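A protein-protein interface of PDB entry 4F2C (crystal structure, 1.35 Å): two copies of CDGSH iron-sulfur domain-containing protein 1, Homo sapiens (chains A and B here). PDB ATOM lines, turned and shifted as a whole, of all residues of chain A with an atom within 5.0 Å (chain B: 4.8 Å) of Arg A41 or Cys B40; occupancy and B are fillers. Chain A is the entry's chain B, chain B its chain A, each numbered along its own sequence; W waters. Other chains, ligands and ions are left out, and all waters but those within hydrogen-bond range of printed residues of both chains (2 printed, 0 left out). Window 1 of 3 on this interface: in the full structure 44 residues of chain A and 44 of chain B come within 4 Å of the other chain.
O of Ile B24 is in hydrogen-bond range of NH2 of Arg A41 (3.0 Å). The backbone carbonyl oxygen of Pro A68 lies within hydrogen-bond range of the backbone NH of His B26 (3.2 Å). ND1 of His B26 is in hydrogen-bond range of NH1 of Arg A41, at 3.1 Å. The indole nitrogen (NE1) of Trp B43 is in hydrogen-bond range of the backbone carbonyl oxygen (O) of Arg A41 (2.8 Å). N of Gly A67 lies within hydrogen-bond range of O of Ile B24 (3.0 Å). The backbone carbonyl oxygen of Arg B41 lies within hydrogen-bond range of the indole nitrogen of Trp A43 (2.8 Å).
The side-chain sulfur of Cys A40 lies close to the backbone NH of Trp A43, 3.3 Å away. N of Trp B43 sits close to SG of Cys B40, 3.3 Å away. The backbone carbonyl oxygen of Leu A69 is in hydrogen-bond range of the backbone NH of Tyr A39, at 2.8 Å. The side-chain hydroxyl of Ser B45 lies within hydrogen-bond range of the backbone NH of Phe B48 (3.5 Å). The guanidinium group of Arg A41 is in hydrogen-bond range of the backbone carbonyl oxygen of Pro A68. NE of Arg A41 is in hydrogen-bond range of O of Gly A67, at 2.8 Å.
Cys A40 touches Arg B41. Val B25 touches Arg A41. Arg A41 touches Cys B40. O of Arg B41 touches O of Arg A41 (3.7 Å). CB of Pro B49 touches NH1 of Arg A41, 3.9 Å away. Ile B13 touches Cys A42 (CD1 to O, 3.0 Å). CZ2 of Trp B43 touches O of Gly A67, at 3.6 Å. Val B25 touches Pro A68 (CA to O, 3.4 Å). Leu A69 touches His B26 (CA to O, 3.4 Å). Tyr B39 touches Leu A69 (CD1 to CD1, 3.4 Å).
Cys B40 touches just one residue of chain A: Arg A41 (3.6 Å). Of the printed residues of chain A, His B26 touches Arg A41, Pro A68 and Leu A69. Printed residues of chain A within 4 Å of Val B25: Arg A41 and Pro A68. Of the printed residues of chain A, Phe B48 touches Arg A41. The nearest residue of chain B that does not touch Arg A41 is Ile B13 (4.6 Å).
Of the 16 printed residues of chain B, 10 touch a printed residue of chain A. Hydrophobic or aromatic side chains of chain B within 4 Å of the printed part of chain A: Ile B13, Ile B24, Val B25, His B26, Tyr B39, Trp B43, Phe B48 and Pro B49.
Cys A40 touches Arg B41, and with the chains exchanged Arg A41 touches Cys B40. Arg B41 touches its own counterpart, Arg A41. Arg A41 touches Trp B43, and with the chains exchanged Trp A43 touches Arg B41. 5 positions are printed for both chains. Of the 17 pairs that touch across the chains among the printed residues, 5 have their exchanged pair printed and touching as well.
Water W2 lies within hydrogen-bond range of O of Cys A40 (2.8 Å) and NH1 of Arg B41 (2.8 Å). Water W1 lies within hydrogen-bond range of the backbone carbonyl oxygen (O) of Cys B40 (2.8 Å), the guanidinium group (NH1) of Arg A41 (2.8 Å) and the backbone carbonyl oxygen (O) of Pro B49 (2.9 Å).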
ATOM      1  N   TYR A  39      30.470 -22.654  -8.531  1.00  0.00           N
ATOM      2  CA  TYR A  39      30.494 -23.259  -9.856  1.00  0.00           C
ATOM      3  C   TYR A  39      29.958 -22.328 -10.929  1.00  0.00           C
ATOM      4  O   TYR A  39      28.924 -21.679 -10.757  1.00  0.00           O
ATOM      5  CB  TYR A  39      29.686 -24.551  -9.854  1.00  0.00           C
ATOM      6  CG  TYR A  39      30.287 -25.606  -8.966  1.00  0.00           C
ATOM      7  CD1 TYR A  39      31.433 -26.294  -9.355  1.00  0.00           C
ATOM      8  CD2 TYR A  39      29.718 -25.924  -7.731  1.00  0.00           C
ATOM      9  CE1 TYR A  39      32.007 -27.252  -8.541  1.00  0.00           C
ATOM     10  CE2 TYR A  39      30.275 -26.905  -6.918  1.00  0.00           C
ATOM     11  CZ  TYR A  39      31.420 -27.568  -7.333  1.00  0.00           C
ATOM     12  OH  TYR A  39      31.976 -28.541  -6.526  1.00  0.00           O
ATOM     13  N   CYS A  40      30.662 -22.274 -12.050  1.00  0.00           N
ATOM     14  CA  CYS A  40      30.300 -21.420 -13.171  1.00  0.00           C
ATOM     15  C   CYS A  40      29.127 -21.969 -13.972  1.00  0.00           C
ATOM     16  O   CYS A  40      29.107 -23.150 -14.355  1.00  0.00           O
ATOM     17  CB  CYS A  40      31.506 -21.266 -14.094  1.00  0.00           C
ATOM     18  SG  CYS A  40      31.219 -20.206 -15.529  1.00  0.00           S
ATOM     19  N   ARG A  41      28.136 -21.117 -14.218  1.00  0.00           N
ATOM     20  CA  ARG A  41      27.023 -21.479 -15.077  1.00  0.00           C
ATOM     21  C   ARG A  41      26.995 -20.602 -16.328  1.00  0.00           C
ATOM     22  O   ARG A  41      26.018 -20.617 -17.070  1.00  0.00           O
ATOM     23  CB  ARG A  41      25.696 -21.380 -14.313  1.00  0.00           C
ATOM     24  CG  ARG A  41      25.632 -22.303 -13.117  1.00  0.00           C
ATOM     25  CD  ARG A  41      24.242 -22.432 -12.534  1.00  0.00           C
ATOM     26  NE  ARG A  41      23.810 -21.167 -11.937  1.00  0.00           N
ATOM     27  CZ  ARG A  41      22.732 -21.046 -11.165  1.00  0.00           C
ATOM     28  NH1 ARG A  41      21.999 -22.113 -10.857  1.00  0.00           N
ATOM     29  NH2 ARG A  41      22.390 -19.864 -10.681  1.00  0.00           N
ATOM     30  N   CYS A  42      28.073 -19.865 -16.587  1.00  0.00           N
ATOM     31  CA  CYS A  42      28.089 -18.927 -17.724  1.00  0.00           C
ATOM     32  C   CYS A  42      29.078 -19.286 -18.837  1.00  0.00           C
ATOM     33  O   CYS A  42      29.062 -18.670 -19.901  1.00  0.00           O
ATOM     34  CB  CYS A  42      28.354 -17.475 -17.264  1.00  0.00           C
ATOM     35  SG  CYS A  42      30.076 -17.104 -16.850  1.00  0.00           S
ATOM     36  N   TRP A  43      29.946 -20.264 -18.590  1.00  0.00           N
ATOM     37  CA  TRP A  43      30.893 -20.737 -19.617  1.00  0.00           C
ATOM     38  C   TRP A  43      31.825 -19.627 -20.090  1.00  0.00           C
ATOM     39  O   TRP A  43      32.302 -19.656 -21.214  1.00  0.00           O
ATOM     40  CB  TRP A  43      30.160 -21.408 -20.807  1.00  0.00           C
ATOM     41  CG  TRP A  43      29.260 -22.504 -20.334  1.00  0.00           C
ATOM     42  CD1 TRP A  43      27.997 -22.368 -19.828  1.00  0.00           C
ATOM     43  CD2 TRP A  43      29.573 -23.894 -20.262  1.00  0.00           C
ATOM     44  NE1 TRP A  43      27.499 -23.596 -19.455  1.00  0.00           N
ATOM     45  CE2 TRP A  43      28.443 -24.553 -19.725  1.00  0.00           C
ATOM     46  CE3 TRP A  43      30.691 -24.653 -20.629  1.00  0.00           C
ATOM     47  CZ2 TRP A  43      28.407 -25.934 -19.524  1.00  0.00           C
ATOM     48  CZ3 TRP A  43      30.654 -26.017 -20.435  1.00  0.00           C
ATOM     49  CH2 TRP A  43      29.522 -26.647 -19.883  1.00  0.00           C
ATOM     50  N   GLY A  67      24.363 -16.193 -13.113  1.00  0.00           N
ATOM     51  CA  GLY A  67      25.255 -16.221 -11.973  1.00  0.00           C
ATOM     52  C   GLY A  67      25.542 -17.659 -11.600  1.00  0.00           C
ATOM     53  O   GLY A  67      24.996 -18.595 -12.193  1.00  0.00           O
ATOM     54  N   PRO A  68      26.425 -17.840 -10.623  1.00  0.00           N
ATOM     55  CA  PRO A  68      26.923 -19.174 -10.282  1.00  0.00           C
ATOM     56  C   PRO A  68      25.990 -19.972  -9.379  1.00  0.00           C
ATOM     57  O   PRO A  68      24.944 -19.493  -8.890  1.00  0.00           O
ATOM     58  CB  PRO A  68      28.224 -18.864  -9.525  1.00  0.00           C
ATOM     59  CG  PRO A  68      27.955 -17.487  -8.898  1.00  0.00           C
ATOM     60  CD  PRO A  68      27.212 -16.768  -9.982  1.00  0.00           C
ATOM     61  N   LEU A  69      26.407 -21.219  -9.188  1.00  0.00           N
ATOM     62  CA  LEU A  69      25.789 -22.108  -8.223  1.00  0.00           C
ATOM     63  C   LEU A  69      26.812 -22.375  -7.138  1.00  0.00           C
ATOM     64  O   LEU A  69      27.943 -22.792  -7.423  1.00  0.00           O
ATOM     65  CB  LEU A  69      25.369 -23.427  -8.870  1.00  0.00           C
ATOM     66  CG  LEU A  69      24.643 -24.372  -7.904  1.00  0.00           C
ATOM     67  CD1 LEU A  69      23.501 -25.056  -8.601  1.00  0.00           C
ATOM     68  CD2 LEU A  69      25.592 -25.398  -7.300  1.00  0.00           C
ATOM     69  N   ILE B  13      23.011 -15.682 -22.635  1.00  0.00           N
ATOM     70  CA  ILE B  13      23.020 -17.112 -22.393  1.00  0.00           C
ATOM     71  C   ILE B  13      21.647 -17.555 -21.913  1.00  0.00           C
ATOM     72  O   ILE B  13      21.096 -18.534 -22.410  1.00  0.00           O
ATOM     73  CB  ILE B  13      24.097 -17.442 -21.352  1.00  0.00           C
ATOM     74  CG1 ILE B  13      25.475 -17.353 -22.027  1.00  0.00           C
ATOM     75  CG2 ILE B  13      23.841 -18.788 -20.696  1.00  0.00           C
ATOM     76  CD1 ILE B  13      26.611 -17.290 -21.052  1.00  0.00           C
ATOM     77  N   ILE B  24      20.963 -14.228 -11.258  1.00  0.00           N
ATOM     78  CA  ILE B  24      20.458 -15.485 -10.738  1.00  0.00           C
ATOM     79  C   ILE B  24      21.575 -16.335 -10.151  1.00  0.00           C
ATOM     80  O   ILE B  24      22.439 -16.847 -10.870  1.00  0.00           O
ATOM     81  CB  ILE B  24      19.688 -16.268 -11.818  1.00  0.00           C
ATOM     82  CG1 ILE B  24      18.488 -15.451 -12.284  1.00  0.00           C
ATOM     83  CG2 ILE B  24      19.221 -17.625 -11.289  1.00  0.00           C
ATOM     84  CD1 ILE B  24      17.888 -15.957 -13.570  1.00  0.00           C
ATOM     85  N   VAL B  25      21.538 -16.474  -8.832  1.00  0.00           N
ATOM     86  CA  VAL B  25      22.507 -17.240  -8.067  1.00  0.00           C
ATOM     87  C   VAL B  25      21.728 -18.251  -7.244  1.00  0.00           C
ATOM     88  O   VAL B  25      20.649 -17.929  -6.716  1.00  0.00           O
ATOM     89  CB  VAL B  25      23.306 -16.324  -7.107  1.00  0.00           C
ATOM     90  CG1 VAL B  25      24.381 -17.118  -6.346  1.00  0.00           C
ATOM     91  CG2 VAL B  25      23.915 -15.137  -7.876  1.00  0.00           C
ATOM     92  N   HIS B  26      22.237 -19.477  -7.167  1.00  0.00           N
ATOM     93  CA  HIS B  26      21.674 -20.470  -6.268  1.00  0.00           C
ATOM     94  C   HIS B  26      22.732 -20.892  -5.281  1.00  0.00           C
ATOM     95  O   HIS B  26      23.896 -21.042  -5.651  1.00  0.00           O
ATOM     96  CB  HIS B  26      21.134 -21.680  -7.035  1.00  0.00           C
ATOM     97  CG  HIS B  26      19.887 -21.362  -7.787  1.00  0.00           C
ATOM     98  ND1 HIS B  26      19.904 -20.811  -9.050  1.00  0.00           N
ATOM     99  CD2 HIS B  26      18.585 -21.432  -7.421  1.00  0.00           C
ATOM    100  CE1 HIS B  26      18.664 -20.585  -9.444  1.00  0.00           C
ATOM    101  NE2 HIS B  26      17.843 -20.957  -8.475  1.00  0.00           N
ATOM    102  N   VAL B  38      21.474 -32.873 -10.045  1.00  0.00           N
ATOM    103  CA  VAL B  38      21.978 -32.602 -11.384  1.00  0.00           C
ATOM    104  C   VAL B  38      21.545 -31.194 -11.723  1.00  0.00           C
ATOM    105  O   VAL B  38      20.353 -30.936 -11.873  1.00  0.00           O
ATOM    106  CB  VAL B  38      21.444 -33.611 -12.422  1.00  0.00           C
ATOM    107  CG1 VAL B  38      22.106 -33.373 -13.777  1.00  0.00           C
ATOM    108  CG2 VAL B  38      21.677 -35.043 -11.946  1.00  0.00           C
ATOM    109  N   TYR B  39      22.514 -30.279 -11.803  1.00  0.00           N
ATOM    110  CA  TYR B  39      22.225 -28.862 -11.930  1.00  0.00           C
ATOM    111  C   TYR B  39      22.437 -28.382 -13.352  1.00  0.00           C
ATOM    112  O   TYR B  39      23.420 -28.747 -14.008  1.00  0.00           O
ATOM    113  CB  TYR B  39      23.114 -28.060 -10.990  1.00  0.00           C
ATOM    114  CG  TYR B  39      22.854 -28.304  -9.526  1.00  0.00           C
ATOM    115  CD1 TYR B  39      21.661 -27.898  -8.935  1.00  0.00           C
ATOM    116  CD2 TYR B  39      23.800 -28.927  -8.730  1.00  0.00           C
ATOM    117  CE1 TYR B  39      21.422 -28.117  -7.586  1.00  0.00           C
ATOM    118  CE2 TYR B  39      23.581 -29.134  -7.377  1.00  0.00           C
ATOM    119  CZ  TYR B  39      22.385 -28.736  -6.809  1.00  0.00           C
ATOM    120  OH  TYR B  39      22.141 -28.934  -5.470  1.00  0.00           O
ATOM    121  N   CYS B  40      21.515 -27.552 -13.816  1.00  0.00           N
ATOM    122  CA  CYS B  40      21.536 -27.038 -15.174  1.00  0.00           C
ATOM    123  C   CYS B  40      22.582 -25.941 -15.387  1.00  0.00           C
ATOM    124  O   CYS B  40      22.696 -25.005 -14.597  1.00  0.00           O
ATOM    125  CB  CYS B  40      20.140 -26.535 -15.533  1.00  0.00           C
ATOM    126  SG  CYS B  40      20.023 -25.803 -17.156  1.00  0.00           S
ATOM    127  N   ARG B  41      23.368 -26.080 -16.449  1.00  0.00           N
ATOM    128  CA  ARG B  41      24.346 -25.062 -16.824  1.00  0.00           C
ATOM    129  C   ARG B  41      24.009 -24.482 -18.189  1.00  0.00           C
ATOM    130  O   ARG B  41      24.798 -23.728 -18.749  1.00  0.00           O
ATOM    131  CB  ARG B  41      25.770 -25.616 -16.792  1.00  0.00           C
ATOM    132  CG  ARG B  41      26.185 -26.119 -15.418  1.00  0.00           C
ATOM    133  CD  ARG B  41      27.684 -26.384 -15.314  1.00  0.00           C
ATOM    134  NE  ARG B  41      28.107 -27.517 -16.153  1.00  0.00           N
ATOM    135  CZ  ARG B  41      29.314 -28.092 -16.085  1.00  0.00           C
ATOM    136  NH1 ARG B  41      30.211 -27.658 -15.205  1.00  0.00           N
ATOM    137  NH2 ARG B  41      29.628 -29.102 -16.903  1.00  0.00           N
ATOM    138  N   CYS B  42      22.828 -24.809 -18.713  1.00  0.00           N
ATOM    139  CA  CYS B  42      22.434 -24.346 -20.050  1.00  0.00           C
ATOM    140  C   CYS B  42      21.285 -23.335 -20.069  1.00  0.00           C
ATOM    141  O   CYS B  42      20.981 -22.770 -21.118  1.00  0.00           O
ATOM    142  CB  CYS B  42      22.092 -25.531 -20.977  1.00  0.00           C
ATOM    143  SG  CYS B  42      20.443 -26.248 -20.680  1.00  0.00           S
ATOM    144  N   TRP B  43      20.650 -23.113 -18.919  1.00  0.00           N
ATOM    145  CA  TRP B  43      19.591 -22.107 -18.806  1.00  0.00           C
ATOM    146  C   TRP B  43      18.439 -22.388 -19.775  1.00  0.00           C
ATOM    147  O   TRP B  43      17.774 -21.461 -20.229  1.00  0.00           O
ATOM    148  CB  TRP B  43      20.147 -20.681 -18.994  1.00  0.00           C
ATOM    149  CG  TRP B  43      21.232 -20.394 -18.010  1.00  0.00           C
ATOM    150  CD1 TRP B  43      22.552 -20.744 -18.120  1.00  0.00           C
ATOM    151  CD2 TRP B  43      21.094 -19.770 -16.730  1.00  0.00           C
ATOM    152  NE1 TRP B  43      23.248 -20.355 -17.011  1.00  0.00           N
ATOM    153  CE2 TRP B  43      22.379 -19.754 -16.133  1.00  0.00           C
ATOM    154  CE3 TRP B  43      20.019 -19.193 -16.041  1.00  0.00           C
ATOM    155  CZ2 TRP B  43      22.613 -19.195 -14.880  1.00  0.00           C
ATOM    156  CZ3 TRP B  43      20.256 -18.628 -14.798  1.00  0.00           C
ATOM    157  CH2 TRP B  43      21.544 -18.622 -14.235  1.00  0.00           C
ATOM    158  N   ARG B  44      18.191 -23.667 -20.073  1.00  0.00           N
ATOM    159  CA  ARG B  44      17.031 -24.048 -20.874  1.00  0.00           C
ATOM    160  C   ARG B  44      16.108 -25.006 -20.127  1.00  0.00           C
ATOM    161  O   ARG B  44      15.034 -25.322 -20.615  1.00  0.00           O
ATOM    162  CB  ARG B  44      17.452 -24.676 -22.201  1.00  0.00           C
ATOM    163  CG  ARG B  44      18.337 -23.795 -23.066  1.00  0.00           C
ATOM    164  CD  ARG B  44      17.569 -22.607 -23.652  1.00  0.00           C
ATOM    165  NE  ARG B  44      18.477 -21.810 -24.473  1.00  0.00           N
ATOM    166  CZ  ARG B  44      19.235 -20.826 -23.998  1.00  0.00           C
ATOM    167  NH1 ARG B  44      19.149 -20.461 -22.714  1.00  0.00           N
ATOM    168  NH2 ARG B  44      20.062 -20.179 -24.806  1.00  0.00           N
ATOM    169  N   SER B  45      16.551 -25.504 -18.974  1.00  0.00           N
ATOM    170  CA  SER B  45      15.704 -26.406 -18.203  1.00  0.00           C
ATOM    171  C   SER B  45      14.384 -25.753 -17.817  1.00  0.00           C
ATOM    172  O   SER B  45      14.350 -24.559 -17.525  1.00  0.00           O
ATOM    173  CB  SER B  45      16.405 -26.860 -16.932  1.00  0.00           C
ATOM    174  OG  SER B  45      15.531 -27.697 -16.203  1.00  0.00           O
ATOM    175  N   PHE B  48      14.702 -25.316 -13.844  1.00  0.00           N
ATOM    176  CA  PHE B  48      15.893 -24.618 -13.363  1.00  0.00           C
ATOM    177  C   PHE B  48      15.736 -24.320 -11.871  1.00  0.00           C
ATOM    178  O   PHE B  48      14.668 -23.876 -11.448  1.00  0.00           O
ATOM    179  CB  PHE B  48      16.108 -23.331 -14.158  1.00  0.00           C
ATOM    180  CG  PHE B  48      17.506 -22.809 -14.075  1.00  0.00           C
ATOM    181  CD1 PHE B  48      18.507 -23.335 -14.899  1.00  0.00           C
ATOM    182  CD2 PHE B  48      17.841 -21.819 -13.162  1.00  0.00           C
ATOM    183  CE1 PHE B  48      19.809 -22.873 -14.818  1.00  0.00           C
ATOM    184  CE2 PHE B  48      19.141 -21.349 -13.068  1.00  0.00           C
ATOM    185  CZ  PHE B  48      20.136 -21.869 -13.895  1.00  0.00           C
ATOM    186  N   PRO B  49      16.793 -24.534 -11.064  1.00  0.00           N
ATOM    187  CA  PRO B  49      18.205 -24.794 -11.388  1.00  0.00           C
ATOM    188  C   PRO B  49      18.569 -26.252 -11.673  1.00  0.00           C
ATOM    189  O   PRO B  49      19.758 -26.536 -11.864  1.00  0.00           O
ATOM    190  CB  PRO B  49      18.917 -24.336 -10.114  1.00  0.00           C
ATOM    191  CG  PRO B  49      17.955 -24.706  -9.022  1.00  0.00           C
ATOM    192  CD  PRO B  49      16.594 -24.394  -9.606  1.00  0.00           C
ATOM    193  N   PHE B  50      17.587 -27.141 -11.731  1.00  0.00           N
ATOM    194  CA  PHE B  50      17.892 -28.546 -11.979  1.00  0.00           C
ATOM    195  C   PHE B  50      17.875 -28.821 -13.460  1.00  0.00           C
ATOM    196  O   PHE B  50      17.157 -28.179 -14.214  1.00  0.00           O
ATOM    197  CB  PHE B  50      16.924 -29.452 -11.213  1.00  0.00           C
ATOM    198  CG  PHE B  50      16.963 -29.208  -9.748  1.00  0.00           C
ATOM    199  CD1 PHE B  50      18.012 -29.696  -8.988  1.00  0.00           C
ATOM    200  CD2 PHE B  50      16.005 -28.419  -9.134  1.00  0.00           C
ATOM    201  CE1 PHE B  50      18.083 -29.437  -7.630  1.00  0.00           C
ATOM    202  CE2 PHE B  50      16.073 -28.163  -7.768  1.00  0.00           C
ATOM    203  CZ  PHE B  50      17.111 -28.664  -7.022  1.00  0.00           C
ATOM    204  N   CYS B  51      18.688 -29.785 -13.866  1.00  0.00           N
ATOM    205  CA  CYS B  51      18.769 -30.215 -15.250  1.00  0.00           C
ATOM    206  C   CYS B  51      17.620 -31.162 -15.567  1.00  0.00           C
ATOM    207  O   CYS B  51      17.387 -32.113 -14.824  1.00  0.00           O
ATOM    208  CB  CYS B  51      20.094 -30.942 -15.444  1.00  0.00           C
ATOM    209  SG  CYS B  51      20.351 -31.735 -17.049  1.00  0.00           S
HETATM  210  O   HOH W   1      21.967 -24.728 -11.926  1.00  0.00           O
HETATM  211  O   HOH W   2      30.244 -25.489 -13.388  1.00  0.00           O
